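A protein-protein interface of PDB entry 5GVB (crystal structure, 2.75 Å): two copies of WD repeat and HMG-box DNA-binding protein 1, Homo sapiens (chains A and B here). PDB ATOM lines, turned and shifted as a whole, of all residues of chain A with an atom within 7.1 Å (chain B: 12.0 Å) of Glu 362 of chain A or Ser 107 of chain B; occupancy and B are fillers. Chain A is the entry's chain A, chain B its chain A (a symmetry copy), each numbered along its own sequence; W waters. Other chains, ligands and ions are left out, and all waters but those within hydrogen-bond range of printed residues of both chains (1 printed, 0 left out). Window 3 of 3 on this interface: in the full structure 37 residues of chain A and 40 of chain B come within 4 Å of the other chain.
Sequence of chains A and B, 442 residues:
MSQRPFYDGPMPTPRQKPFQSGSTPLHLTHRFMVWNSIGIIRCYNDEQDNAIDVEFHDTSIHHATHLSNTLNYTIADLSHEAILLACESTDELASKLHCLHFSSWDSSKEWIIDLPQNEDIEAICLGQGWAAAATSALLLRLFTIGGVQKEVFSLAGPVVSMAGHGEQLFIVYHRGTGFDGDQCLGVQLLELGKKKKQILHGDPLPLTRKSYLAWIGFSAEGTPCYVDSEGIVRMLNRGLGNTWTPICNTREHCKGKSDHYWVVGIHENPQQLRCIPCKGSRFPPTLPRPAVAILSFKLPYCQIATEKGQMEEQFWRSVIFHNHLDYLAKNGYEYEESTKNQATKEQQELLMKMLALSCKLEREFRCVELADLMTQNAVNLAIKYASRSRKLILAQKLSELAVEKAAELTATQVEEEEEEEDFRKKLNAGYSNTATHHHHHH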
ATOM      1  N   ALA A 356      -8.306 -31.489  15.582  1.00  0.00           N
ATOM      2  CA  ALA A 356      -8.032 -31.202  14.179  1.00  0.00           C
ATOM      3  C   ALA A 356      -9.328 -31.112  13.383  1.00  0.00           C
ATOM      4  O   ALA A 356      -9.537 -30.167  12.611  1.00  0.00           O
ATOM      5  CB  ALA A 356      -7.110 -32.272  13.595  1.00  0.00           C
ATOM      6  N   LEU A 357     -10.216 -32.089  13.573  1.00  0.00           N
ATOM      7  CA  LEU A 357     -11.510 -32.072  12.899  1.00  0.00           C
ATOM      8  C   LEU A 357     -12.283 -30.804  13.242  1.00  0.00           C
ATOM      9  O   LEU A 357     -12.765 -30.099  12.350  1.00  0.00           O
ATOM     10  CB  LEU A 357     -12.309 -33.317  13.283  1.00  0.00           C
ATOM     11  CG  LEU A 357     -13.665 -33.504  12.595  1.00  0.00           C
ATOM     12  CD1 LEU A 357     -13.466 -34.053  11.194  1.00  0.00           C
ATOM     13  CD2 LEU A 357     -14.571 -34.413  13.404  1.00  0.00           C
ATOM     14  N   SER A 358     -12.388 -30.487  14.534  1.00  0.00           N
ATOM     15  CA  SER A 358     -13.077 -29.271  14.952  1.00  0.00           C
ATOM     16  C   SER A 358     -12.415 -28.024  14.378  1.00  0.00           C
ATOM     17  O   SER A 358     -13.094 -27.024  14.116  1.00  0.00           O
ATOM     18  CB  SER A 358     -13.121 -29.198  16.478  1.00  0.00           C
ATOM     19  OG  SER A 358     -13.814 -28.043  16.918  1.00  0.00           O
ATOM     20  N   CYS A 359     -11.098 -28.069  14.163  1.00  0.00           N
ATOM     21  CA  CYS A 359     -10.384 -26.907  13.644  1.00  0.00           C
ATOM     22  C   CYS A 359     -10.667 -26.698  12.162  1.00  0.00           C
ATOM     23  O   CYS A 359     -10.808 -25.556  11.708  1.00  0.00           O
ATOM     24  CB  CYS A 359      -8.883 -27.066  13.891  1.00  0.00           C
ATOM     25  SG  CYS A 359      -7.888 -25.624  13.457  1.00  0.00           S
ATOM     26  N   LYS A 360     -10.755 -27.784  11.390  1.00  0.00           N
ATOM     27  CA  LYS A 360     -11.082 -27.657   9.974  1.00  0.00           C
ATOM     28  C   LYS A 360     -12.504 -27.166   9.738  1.00  0.00           C
ATOM     29  O   LYS A 360     -12.839 -26.812   8.603  1.00  0.00           O
ATOM     30  CB  LYS A 360     -10.869 -28.990   9.258  1.00  0.00           C
ATOM     31  CG  LYS A 360      -9.426 -29.461   9.269  1.00  0.00           C
ATOM     32  CD  LYS A 360      -9.213 -30.636   8.331  1.00  0.00           C
ATOM     33  CE  LYS A 360      -7.746 -31.031   8.284  1.00  0.00           C
ATOM     34  NZ  LYS A 360      -7.479 -32.088   7.272  1.00  0.00           N
ATOM     35  N   LEU A 361     -13.342 -27.142  10.773  1.00  0.00           N
ATOM     36  CA  LEU A 361     -14.692 -26.604  10.698  1.00  0.00           C
ATOM     37  C   LEU A 361     -14.787 -25.202  11.287  1.00  0.00           C
ATOM     38  O   LEU A 361     -15.896 -24.687  11.464  1.00  0.00           O
ATOM     39  CB  LEU A 361     -15.678 -27.545  11.400  1.00  0.00           C
ATOM     40  CG  LEU A 361     -16.103 -28.886  10.771  1.00  0.00           C
ATOM     41  CD1 LEU A 361     -14.951 -29.755  10.272  1.00  0.00           C
ATOM     42  CD2 LEU A 361     -16.947 -29.668  11.771  1.00  0.00           C
ATOM     43  N   GLU A 362     -13.644 -24.580  11.593  1.00  0.00           N
ATOM     44  CA  GLU A 362     -13.581 -23.222  12.141  1.00  0.00           C
ATOM     45  C   GLU A 362     -14.431 -23.072  13.401  1.00  0.00           C
ATOM     46  O   GLU A 362     -14.960 -21.995  13.689  1.00  0.00           O
ATOM     47  CB  GLU A 362     -13.969 -22.179  11.089  1.00  0.00           C
ATOM     48  CG  GLU A 362     -13.181 -22.312   9.795  1.00  0.00           C
ATOM     49  CD  GLU A 362     -13.906 -21.732   8.599  1.00  0.00           C
ATOM     50  OE1 GLU A 362     -14.789 -20.871   8.797  1.00  0.00           O
ATOM     51  OE2 GLU A 362     -13.590 -22.136   7.459  1.00  0.00           O
ATOM     52  N   ARG A 363     -14.564 -24.156  14.162  1.00  0.00           N
ATOM     53  CA  ARG A 363     -15.145 -24.116  15.502  1.00  0.00           C
ATOM     54  C   ARG A 363     -13.975 -24.184  16.477  1.00  0.00           C
ATOM     55  O   ARG A 363     -13.595 -25.254  16.953  1.00  0.00           O
ATOM     56  CB  ARG A 363     -16.138 -25.253  15.719  1.00  0.00           C
ATOM     57  CG  ARG A 363     -17.157 -25.407  14.606  1.00  0.00           C
ATOM     58  CD  ARG A 363     -18.240 -26.398  14.988  1.00  0.00           C
ATOM     59  NE  ARG A 363     -19.455 -25.715  15.419  1.00  0.00           N
ATOM     60  CZ  ARG A 363     -20.583 -25.690  14.719  1.00  0.00           C
ATOM     61  NH1 ARG A 363     -20.652 -26.314  13.551  1.00  0.00           N
ATOM     62  NH2 ARG A 363     -21.640 -25.042  15.184  1.00  0.00           N
ATOM     63  N   GLU A 364     -13.393 -23.020  16.764  1.00  0.00           N
ATOM     64  CA  GLU A 364     -12.167 -22.965  17.549  1.00  0.00           C
ATOM     65  C   GLU A 364     -12.444 -23.003  19.049  1.00  0.00           C
ATOM     66  O   GLU A 364     -11.624 -23.527  19.818  1.00  0.00           O
ATOM     67  CB  GLU A 364     -11.382 -21.712  17.157  1.00  0.00           C
ATOM     68  CG  GLU A 364     -11.388 -21.454  15.650  1.00  0.00           C
ATOM     69  CD  GLU A 364     -10.704 -20.159  15.258  1.00  0.00           C
ATOM     70  OE1 GLU A 364     -10.409 -19.340  16.153  1.00  0.00           O
ATOM     71  OE2 GLU A 364     -10.467 -19.957  14.048  1.00  0.00           O
ATOM     72  N   PHE A 365     -13.589 -22.467  19.480  1.00  0.00           N
ATOM     73  CA  PHE A 365     -13.994 -22.613  20.874  1.00  0.00           C
ATOM     74  C   PHE A 365     -14.115 -24.083  21.252  1.00  0.00           C
ATOM     75  O   PHE A 365     -13.674 -24.498  22.333  1.00  0.00           O
ATOM     76  CB  PHE A 365     -15.318 -21.884  21.111  1.00  0.00           C
ATOM     77  CG  PHE A 365     -15.758 -21.880  22.544  1.00  0.00           C
ATOM     78  CD1 PHE A 365     -15.305 -20.902  23.414  1.00  0.00           C
ATOM     79  CD2 PHE A 365     -16.617 -22.853  23.027  1.00  0.00           C
ATOM     80  CE1 PHE A 365     -15.702 -20.892  24.736  1.00  0.00           C
ATOM     81  CE2 PHE A 365     -17.017 -22.849  24.350  1.00  0.00           C
ATOM     82  CZ  PHE A 365     -16.559 -21.867  25.206  1.00  0.00           C
ATOM     83  N   CYS A 367     -12.445 -26.433  19.892  1.00  0.00           N
ATOM     84  CA  CYS A 367     -11.067 -26.905  19.984  1.00  0.00           C
ATOM     85  C   CYS A 367     -10.494 -26.651  21.373  1.00  0.00           C
ATOM     86  O   CYS A 367      -9.874 -27.538  21.972  1.00  0.00           O
ATOM     87  CB  CYS A 367     -10.202 -26.232  18.918  1.00  0.00           C
ATOM     88  SG  CYS A 367     -10.666 -26.608  17.215  1.00  0.00           S
ATOM     89  N   LYS A 391      -5.159 -20.477  12.985  1.00  0.00           N
ATOM     90  CA  LYS A 391      -6.019 -19.750  13.907  1.00  0.00           C
ATOM     91  C   LYS A 391      -5.086 -19.219  14.989  1.00  0.00           C
ATOM     92  O   LYS A 391      -4.738 -19.915  15.943  1.00  0.00           O
ATOM     93  CB  LYS A 391      -7.116 -20.654  14.456  1.00  0.00           C
ATOM     94  CG  LYS A 391      -7.536 -21.760  13.497  1.00  0.00           C
ATOM     95  CD  LYS A 391      -8.392 -21.221  12.364  1.00  0.00           C
ATOM     96  CE  LYS A 391      -8.905 -22.347  11.485  1.00  0.00           C
ATOM     97  NZ  LYS A 391     -10.060 -21.926  10.647  1.00  0.00           N
ATOM     98  N   HIS B  62     -26.023  -9.245  26.062  1.00  0.00           N
ATOM     99  CA  HIS B  62     -26.233  -9.647  24.678  1.00  0.00           C
ATOM    100  C   HIS B  62     -27.364  -8.810  24.100  1.00  0.00           C
ATOM    101  O   HIS B  62     -28.186  -8.257  24.835  1.00  0.00           O
ATOM    102  CB  HIS B  62     -26.555 -11.142  24.568  1.00  0.00           C
ATOM    103  CG  HIS B  62     -26.280 -11.718  23.215  1.00  0.00           C
ATOM    104  ND1 HIS B  62     -25.022 -11.718  22.652  1.00  0.00           N
ATOM    105  CD2 HIS B  62     -27.096 -12.318  22.316  1.00  0.00           C
ATOM    106  CE1 HIS B  62     -25.076 -12.284  21.460  1.00  0.00           C
ATOM    107  NE2 HIS B  62     -26.322 -12.662  21.233  1.00  0.00           N
ATOM    108  N   HIS B  63     -27.389  -8.717  22.773  1.00  0.00           N
ATOM    109  CA  HIS B  63     -28.468  -8.016  22.097  1.00  0.00           C
ATOM    110  C   HIS B  63     -29.699  -8.911  22.017  1.00  0.00           C
ATOM    111  O   HIS B  63     -29.600 -10.141  22.058  1.00  0.00           O
ATOM    112  CB  HIS B  63     -28.041  -7.575  20.695  1.00  0.00           C
ATOM    113  CG  HIS B  63     -28.029  -8.681  19.683  1.00  0.00           C
ATOM    114  ND1 HIS B  63     -27.210  -9.784  19.792  1.00  0.00           N
ATOM    115  CD2 HIS B  63     -28.727  -8.844  18.534  1.00  0.00           C
ATOM    116  CE1 HIS B  63     -27.411 -10.584  18.760  1.00  0.00           C
ATOM    117  NE2 HIS B  63     -28.326 -10.037  17.981  1.00  0.00           N
ATOM    118  N   GLU B  81     -24.290 -17.167  28.761  1.00  0.00           N
ATOM    119  CA  GLU B  81     -23.371 -17.476  27.676  1.00  0.00           C
ATOM    120  C   GLU B  81     -23.984 -18.241  26.512  1.00  0.00           C
ATOM    121  O   GLU B  81     -23.309 -18.376  25.486  1.00  0.00           O
ATOM    122  CB  GLU B  81     -22.165 -18.265  28.213  1.00  0.00           C
ATOM    123  CG  GLU B  81     -22.503 -19.602  28.853  1.00  0.00           C
ATOM    124  CD  GLU B  81     -21.305 -20.227  29.550  1.00  0.00           C
ATOM    125  OE1 GLU B  81     -20.299 -19.515  29.759  1.00  0.00           O
ATOM    126  OE2 GLU B  81     -21.365 -21.428  29.884  1.00  0.00           O
ATOM    127  N   HIS B  98     -30.360 -27.985  20.198  1.00  0.00           N
ATOM    128  CA  HIS B  98     -29.810 -26.867  19.450  1.00  0.00           C
ATOM    129  C   HIS B  98     -29.262 -25.845  20.433  1.00  0.00           C
ATOM    130  O   HIS B  98     -29.880 -25.577  21.466  1.00  0.00           O
ATOM    131  CB  HIS B  98     -30.894 -26.242  18.558  1.00  0.00           C
ATOM    132  CG  HIS B  98     -30.438 -25.057  17.765  1.00  0.00           C
ATOM    133  ND1 HIS B  98     -29.223 -25.014  17.116  1.00  0.00           N
ATOM    134  CD2 HIS B  98     -31.051 -23.882  17.492  1.00  0.00           C
ATOM    135  CE1 HIS B  98     -29.101 -23.856  16.490  1.00  0.00           C
ATOM    136  NE2 HIS B  98     -30.198 -23.152  16.700  1.00  0.00           N
ATOM    137  N   CYS B  99     -28.098 -25.282  20.123  1.00  0.00           N
ATOM    138  CA  CYS B  99     -27.460 -24.339  21.029  1.00  0.00           C
ATOM    139  C   CYS B  99     -26.887 -23.159  20.265  1.00  0.00           C
ATOM    140  O   CYS B  99     -26.182 -23.336  19.266  1.00  0.00           O
ATOM    141  CB  CYS B  99     -26.352 -25.007  21.847  1.00  0.00           C
ATOM    142  SG  CYS B  99     -25.458 -23.881  22.948  1.00  0.00           S
ATOM    143  N   LEU B 100     -27.197 -21.957  20.738  1.00  0.00           N
ATOM    144  CA  LEU B 100     -26.599 -20.716  20.259  1.00  0.00           C
ATOM    145  C   LEU B 100     -25.703 -20.200  21.381  1.00  0.00           C
ATOM    146  O   LEU B 100     -26.146 -19.436  22.240  1.00  0.00           O
ATOM    147  CB  LEU B 100     -27.660 -19.677  19.887  1.00  0.00           C
ATOM    148  CG  LEU B 100     -28.564 -19.860  18.667  1.00  0.00           C
ATOM    149  CD1 LEU B 100     -29.690 -20.840  18.954  1.00  0.00           C
ATOM    150  CD2 LEU B 100     -29.120 -18.513  18.236  1.00  0.00           C
ATOM    151  N   HIS B 101     -24.445 -20.632  21.386  1.00  0.00           N
ATOM    152  CA  HIS B 101     -23.487 -20.126  22.366  1.00  0.00           C
ATOM    153  C   HIS B 101     -22.866 -18.865  21.774  1.00  0.00           C
ATOM    154  O   HIS B 101     -21.966 -18.923  20.932  1.00  0.00           O
ATOM    155  CB  HIS B 101     -22.470 -21.198  22.763  1.00  0.00           C
ATOM    156  CG  HIS B 101     -21.453 -21.528  21.714  1.00  0.00           C
ATOM    157  ND1 HIS B 101     -21.785 -22.022  20.472  1.00  0.00           N
ATOM    158  CD2 HIS B 101     -20.100 -21.462  21.742  1.00  0.00           C
ATOM    159  CE1 HIS B 101     -20.683 -22.230  19.774  1.00  0.00           C
ATOM    160  NE2 HIS B 101     -19.646 -21.896  20.521  1.00  0.00           N
ATOM    161  N   PHE B 102     -23.389 -17.712  22.196  1.00  0.00           N
ATOM    162  CA  PHE B 102     -23.013 -16.438  21.594  1.00  0.00           C
ATOM    163  C   PHE B 102     -21.745 -15.861  22.202  1.00  0.00           C
ATOM    164  O   PHE B 102     -20.978 -15.192  21.501  1.00  0.00           O
ATOM    165  CB  PHE B 102     -24.161 -15.440  21.735  1.00  0.00           C
ATOM    166  CG  PHE B 102     -24.821 -15.455  23.086  1.00  0.00           C
ATOM    167  CD1 PHE B 102     -24.266 -14.772  24.155  1.00  0.00           C
ATOM    168  CD2 PHE B 102     -26.005 -16.148  23.283  1.00  0.00           C
ATOM    169  CE1 PHE B 102     -24.873 -14.787  25.398  1.00  0.00           C
ATOM    170  CE2 PHE B 102     -26.619 -16.164  24.521  1.00  0.00           C
ATOM    171  CZ  PHE B 102     -26.052 -15.483  25.581  1.00  0.00           C
ATOM    172  N   SER B 103     -21.505 -16.110  23.492  1.00  0.00           N
ATOM    173  CA  SER B 103     -20.316 -15.593  24.159  1.00  0.00           C
ATOM    174  C   SER B 103     -19.026 -16.134  23.562  1.00  0.00           C
ATOM    175  O   SER B 103     -17.944 -15.703  23.976  1.00  0.00           O
ATOM    176  CB  SER B 103     -20.372 -15.931  25.647  1.00  0.00           C
ATOM    177  OG  SER B 103     -20.439 -17.332  25.831  1.00  0.00           O
ATOM    178  N   SER B 104     -19.111 -17.064  22.616  1.00  0.00           N
ATOM    179  CA  SER B 104     -17.921 -17.598  21.976  1.00  0.00           C
ATOM    180  C   SER B 104     -17.209 -16.518  21.171  1.00  0.00           C
ATOM    181  O   SER B 104     -17.831 -15.624  20.592  1.00  0.00           O
ATOM    182  CB  SER B 104     -18.283 -18.770  21.067  1.00  0.00           C
ATOM    183  OG  SER B 104     -19.133 -18.355  20.011  1.00  0.00           O
ATOM    184  N   TRP B 105     -15.886 -16.617  21.142  1.00  0.00           N
ATOM    185  CA  TRP B 105     -15.029 -15.675  20.443  1.00  0.00           C
ATOM    186  C   TRP B 105     -14.806 -16.039  18.982  1.00  0.00           C
ATOM    187  O   TRP B 105     -14.192 -15.255  18.251  1.00  0.00           O
ATOM    188  CB  TRP B 105     -13.682 -15.590  21.162  1.00  0.00           C
ATOM    189  CG  TRP B 105     -13.219 -16.934  21.628  1.00  0.00           C
ATOM    190  CD1 TRP B 105     -13.510 -17.536  22.819  1.00  0.00           C
ATOM    191  CD2 TRP B 105     -12.404 -17.859  20.901  1.00  0.00           C
ATOM    192  NE1 TRP B 105     -12.919 -18.773  22.881  1.00  0.00           N
ATOM    193  CE2 TRP B 105     -12.235 -18.996  21.716  1.00  0.00           C
ATOM    194  CE3 TRP B 105     -11.796 -17.835  19.643  1.00  0.00           C
ATOM    195  CZ2 TRP B 105     -11.480 -20.094  21.316  1.00  0.00           C
ATOM    196  CZ3 TRP B 105     -11.050 -18.926  19.247  1.00  0.00           C
ATOM    197  CH2 TRP B 105     -10.897 -20.040  20.082  1.00  0.00           C
ATOM    198  N   ASP B 106     -15.282 -17.200  18.542  1.00  0.00           N
ATOM    199  CA  ASP B 106     -15.060 -17.673  17.184  1.00  0.00           C
ATOM    200  C   ASP B 106     -16.263 -17.361  16.298  1.00  0.00           C
ATOM    201  O   ASP B 106     -17.320 -16.927  16.761  1.00  0.00           O
ATOM    202  CB  ASP B 106     -14.765 -19.178  17.181  1.00  0.00           C
ATOM    203  CG  ASP B 106     -15.937 -20.006  17.667  1.00  0.00           C
ATOM    204  OD1 ASP B 106     -16.771 -19.472  18.427  1.00  0.00           O
ATOM    205  OD2 ASP B 106     -16.024 -21.195  17.292  1.00  0.00           O
ATOM    206  N   SER B 107     -16.081 -17.597  14.997  1.00  0.00           N
ATOM    207  CA  SER B 107     -17.131 -17.289  14.030  1.00  0.00           C
ATOM    208  C   SER B 107     -18.312 -18.244  14.170  1.00  0.00           C
ATOM    209  O   SER B 107     -19.460 -17.807  14.306  1.00  0.00           O
ATOM    210  CB  SER B 107     -16.562 -17.338  12.612  1.00  0.00           C
ATOM    211  OG  SER B 107     -15.968 -18.596  12.345  1.00  0.00           O
ATOM    212  N   SER B 108     -18.048 -19.550  14.130  1.00  0.00           N
ATOM    213  CA  SER B 108     -19.113 -20.541  14.238  1.00  0.00           C
ATOM    214  C   SER B 108     -19.822 -20.411  15.580  1.00  0.00           C
ATOM    215  O   SER B 108     -19.201 -20.547  16.638  1.00  0.00           O
ATOM    216  CB  SER B 108     -18.537 -21.946  14.061  1.00  0.00           C
ATOM    217  OG  SER B 108     -17.988 -22.109  12.765  1.00  0.00           O
ATOM    218  N   LYS B 109     -21.129 -20.160  15.532  1.00  0.00           N
ATOM    219  CA  LYS B 109     -21.891 -19.698  16.688  1.00  0.00           C
ATOM    220  C   LYS B 109     -22.868 -20.723  17.242  1.00  0.00           C
ATOM    221  O   LYS B 109     -22.990 -20.848  18.462  1.00  0.00           O
ATOM    222  CB  LYS B 109     -22.655 -18.421  16.316  1.00  0.00           C
ATOM    223  CG  LYS B 109     -22.975 -17.501  17.481  1.00  0.00           C
ATOM    224  CD  LYS B 109     -24.352 -17.775  18.057  1.00  0.00           C
ATOM    225  CE  LYS B 109     -25.021 -16.480  18.481  1.00  0.00           C
ATOM    226  NZ  LYS B 109     -26.230 -16.714  19.317  1.00  0.00           N
ATOM    227  N   GLU B 110     -23.576 -21.453  16.386  1.00  0.00           N
ATOM    228  CA  GLU B 110     -24.606 -22.389  16.811  1.00  0.00           C
ATOM    229  C   GLU B 110     -24.270 -23.805  16.368  1.00  0.00           C
ATOM    230  O   GLU B 110     -23.627 -24.017  15.335  1.00  0.00           O
ATOM    231  CB  GLU B 110     -25.976 -21.992  16.248  1.00  0.00           C
ATOM    232  CG  GLU B 110     -25.982 -21.766  14.744  1.00  0.00           C
ATOM    233  CD  GLU B 110     -27.375 -21.536  14.193  1.00  0.00           C
ATOM    234  OE1 GLU B 110     -27.989 -22.505  13.701  1.00  0.00           O
ATOM    235  OE2 GLU B 110     -27.858 -20.384  14.255  1.00  0.00           O
ATOM    236  N   TRP B 111     -24.716 -24.779  17.161  1.00  0.00           N
ATOM    237  CA  TRP B 111     -24.637 -26.182  16.781  1.00  0.00           C
ATOM    238  C   TRP B 111     -25.977 -26.849  17.051  1.00  0.00           C
ATOM    239  O   TRP B 111     -26.830 -26.311  17.759  1.00  0.00           O
ATOM    240  CB  TRP B 111     -23.510 -26.927  17.521  1.00  0.00           C
ATOM    241  CG  TRP B 111     -23.580 -26.875  19.025  1.00  0.00           C
ATOM    242  CD1 TRP B 111     -22.913 -26.011  19.845  1.00  0.00           C
ATOM    243  CD2 TRP B 111     -24.339 -27.737  19.885  1.00  0.00           C
ATOM    244  NE1 TRP B 111     -23.218 -26.275  21.159  1.00  0.00           N
ATOM    245  CE2 TRP B 111     -24.088 -27.331  21.211  1.00  0.00           C
ATOM    246  CE3 TRP B 111     -25.208 -28.810  19.662  1.00  0.00           C
ATOM    247  CZ2 TRP B 111     -24.678 -27.957  22.308  1.00  0.00           C
ATOM    248  CZ3 TRP B 111     -25.792 -29.429  20.754  1.00  0.00           C
ATOM    249  CH2 TRP B 111     -25.525 -29.001  22.059  1.00  0.00           C
ATOM    250  N   ILE B 145     -20.873 -26.491  25.833  1.00  0.00           N
ATOM    251  CA  ILE B 145     -21.653 -25.490  25.114  1.00  0.00           C
ATOM    252  C   ILE B 145     -21.192 -25.383  23.669  1.00  0.00           C
ATOM    253  O   ILE B 145     -21.956 -24.936  22.807  1.00  0.00           O
ATOM    254  CB  ILE B 145     -21.590 -24.119  25.818  1.00  0.00           C
ATOM    255  CG1 ILE B 145     -20.143 -23.730  26.126  1.00  0.00           C
ATOM    256  CG2 ILE B 145     -22.444 -24.125  27.080  1.00  0.00           C
ATOM    257  CD1 ILE B 145     -20.011 -22.387  26.816  1.00  0.00           C
ATOM    258  N   GLY B 146     -19.961 -25.802  23.379  1.00  0.00           N
ATOM    259  CA  GLY B 146     -19.429 -25.843  22.034  1.00  0.00           C
ATOM    260  C   GLY B 146     -19.811 -27.055  21.216  1.00  0.00           C
ATOM    261  O   GLY B 146     -19.410 -27.152  20.053  1.00  0.00           O
ATOM    262  N   GLY B 147     -20.561 -27.994  21.785  1.00  0.00           N
ATOM    263  CA  GLY B 147     -21.106 -29.102  21.031  1.00  0.00           C
ATOM    264  C   GLY B 147     -20.393 -30.431  21.163  1.00  0.00           C
ATOM    265  O   GLY B 147     -20.666 -31.333  20.363  1.00  0.00           O
ATOM    266  N   VAL B 148     -19.498 -30.587  22.132  1.00  0.00           N
ATOM    267  CA  VAL B 148     -18.811 -31.855  22.351  1.00  0.00           C
ATOM    268  C   VAL B 148     -19.671 -32.722  23.259  1.00  0.00           C
ATOM    269  O   VAL B 148     -20.036 -32.307  24.364  1.00  0.00           O
ATOM    270  CB  VAL B 148     -17.417 -31.644  22.961  1.00  0.00           C
ATOM    271  CG1 VAL B 148     -16.793 -32.985  23.326  1.00  0.00           C
ATOM    272  CG2 VAL B 148     -16.526 -30.887  22.000  1.00  0.00           C
HETATM  273  O   HOH W   1     -19.547 -24.760  17.977  1.00  0.00           O
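The backbone carbonyl oxygen (O) of Glu 110 of chain B lies close to the guanidinium group (NH2) of Arg 363 of chain A, 2.2 Å away.
The backbone carbonyl oxygen of Glu 362 of chain A is in hydrogen-bond range of the side-chain hydroxyl of Ser 108 of chain B (3.2 Å).
The backbone NH of Glu 364 of chain A is in hydrogen-bond range of the side-chain carboxylate of Asp 106 of chain B.
The backbone NH (N) of Cys 99 of chain B lies within hydrogen-bond range of the backbone carbonyl oxygen (O) of Trp 111 of chain B (2.9 Å).
OE2 of Glu 364 of chain A is in salt-bridge range of NZ of Lys 391 of chain A, at 3.95 Å.
O of Trp 111 of chain B sits at hydrogen-bond distance from ND1 of His 98 of chain B (2.8 Å).
O of Arg 363 of chain A sits at hydrogen-bond distance from SG of Cys 367 of chain A (3.2 Å).
The side-chain hydroxyl (OG) of Ser 104 of chain B sits at hydrogen-bond distance from the side-chain carboxylate (OD1) of Asp 106 of chain B (3.1 Å).
O of Ile 145 of chain B is in hydrogen-bond range of SG of Cys 99 of chain B, at 3.7 Å.
Hydrophobic or aromatic side chains of chain A that line the printed part of chain B: Phe 365.
Of the 21 printed residues of chain B, 8 touch a printed residue of chain A.
Among the printed residues, pairs that only touch across the chains: Leu 361 of chain A with Ser 108 of chain B (3.6 Å), Glu 362 of chain A with Asp 106 of chain B (3.8 Å), Glu 362 of chain A with Ser 107 of chain B (3.8 Å), Arg 363 of chain A with Asp 106 of chain B (3.5 Å), Arg 363 of chain A with Ser 108 of chain B (3.8 Å), Arg 363 of chain A with Trp 111 of chain B (3.5 Å), Glu 364 of chain A with Trp 105 of chain B (3.2 Å), Phe 365 of chain A with His 101 of chain B (3.96 Å), Phe 365 of chain A with Trp 105 of chain B (3.2 Å), Phe 365 of chain A with Asp 106 of chain B (3.5 Å) and Phe 365 of chain A with Ile 145 of chain B (3.7 Å).
No position is printed for both chains.
Of the printed residues of chain B, Glu 362 of chain A touches Asp 106, Ser 107 and Ser 108.
Of the printed residues of chain A, Ser 107 of chain B touches Glu 362 (3.8 Å).
No residue of chain B comes within 4 Å of Ser 358 of chain A.
Printed residues of chain A within 4 Å of Trp 105 of chain B: Glu 364 (3.2 Å) and Phe 365 (3.2 Å).
Printed residues of chain A within 4 Å of Trp 111 of chain B: Arg 363.
Of the printed residues of chain A, Glu 110 of chain B touches Arg 363.
Printed residues of chain A within 4 Å of Asp 106 of chain B: Glu 362 (3.8 Å), Arg 363 (3.5 Å), Glu 364 (3.2 Å) and Phe 365 (3.5 Å).
Printed residues of chain B within 4 Å of Arg 363 of chain A: Asp 106, Ser 108, Glu 110 and Trp 111.
His 62 of chain B touches none of the printed residues of chain A.
The nearest printed residue of chain A that does not touch Ser 107 of chain B is Glu 364 of chain A (5.9 Å).
Water W1 lies within hydrogen-bond range of the guanidinium group (NE) of Arg 363 of chain A (2.7 Å) and the backbone carbonyl oxygen (O) of Gly 146 of chain B (3.2 Å).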
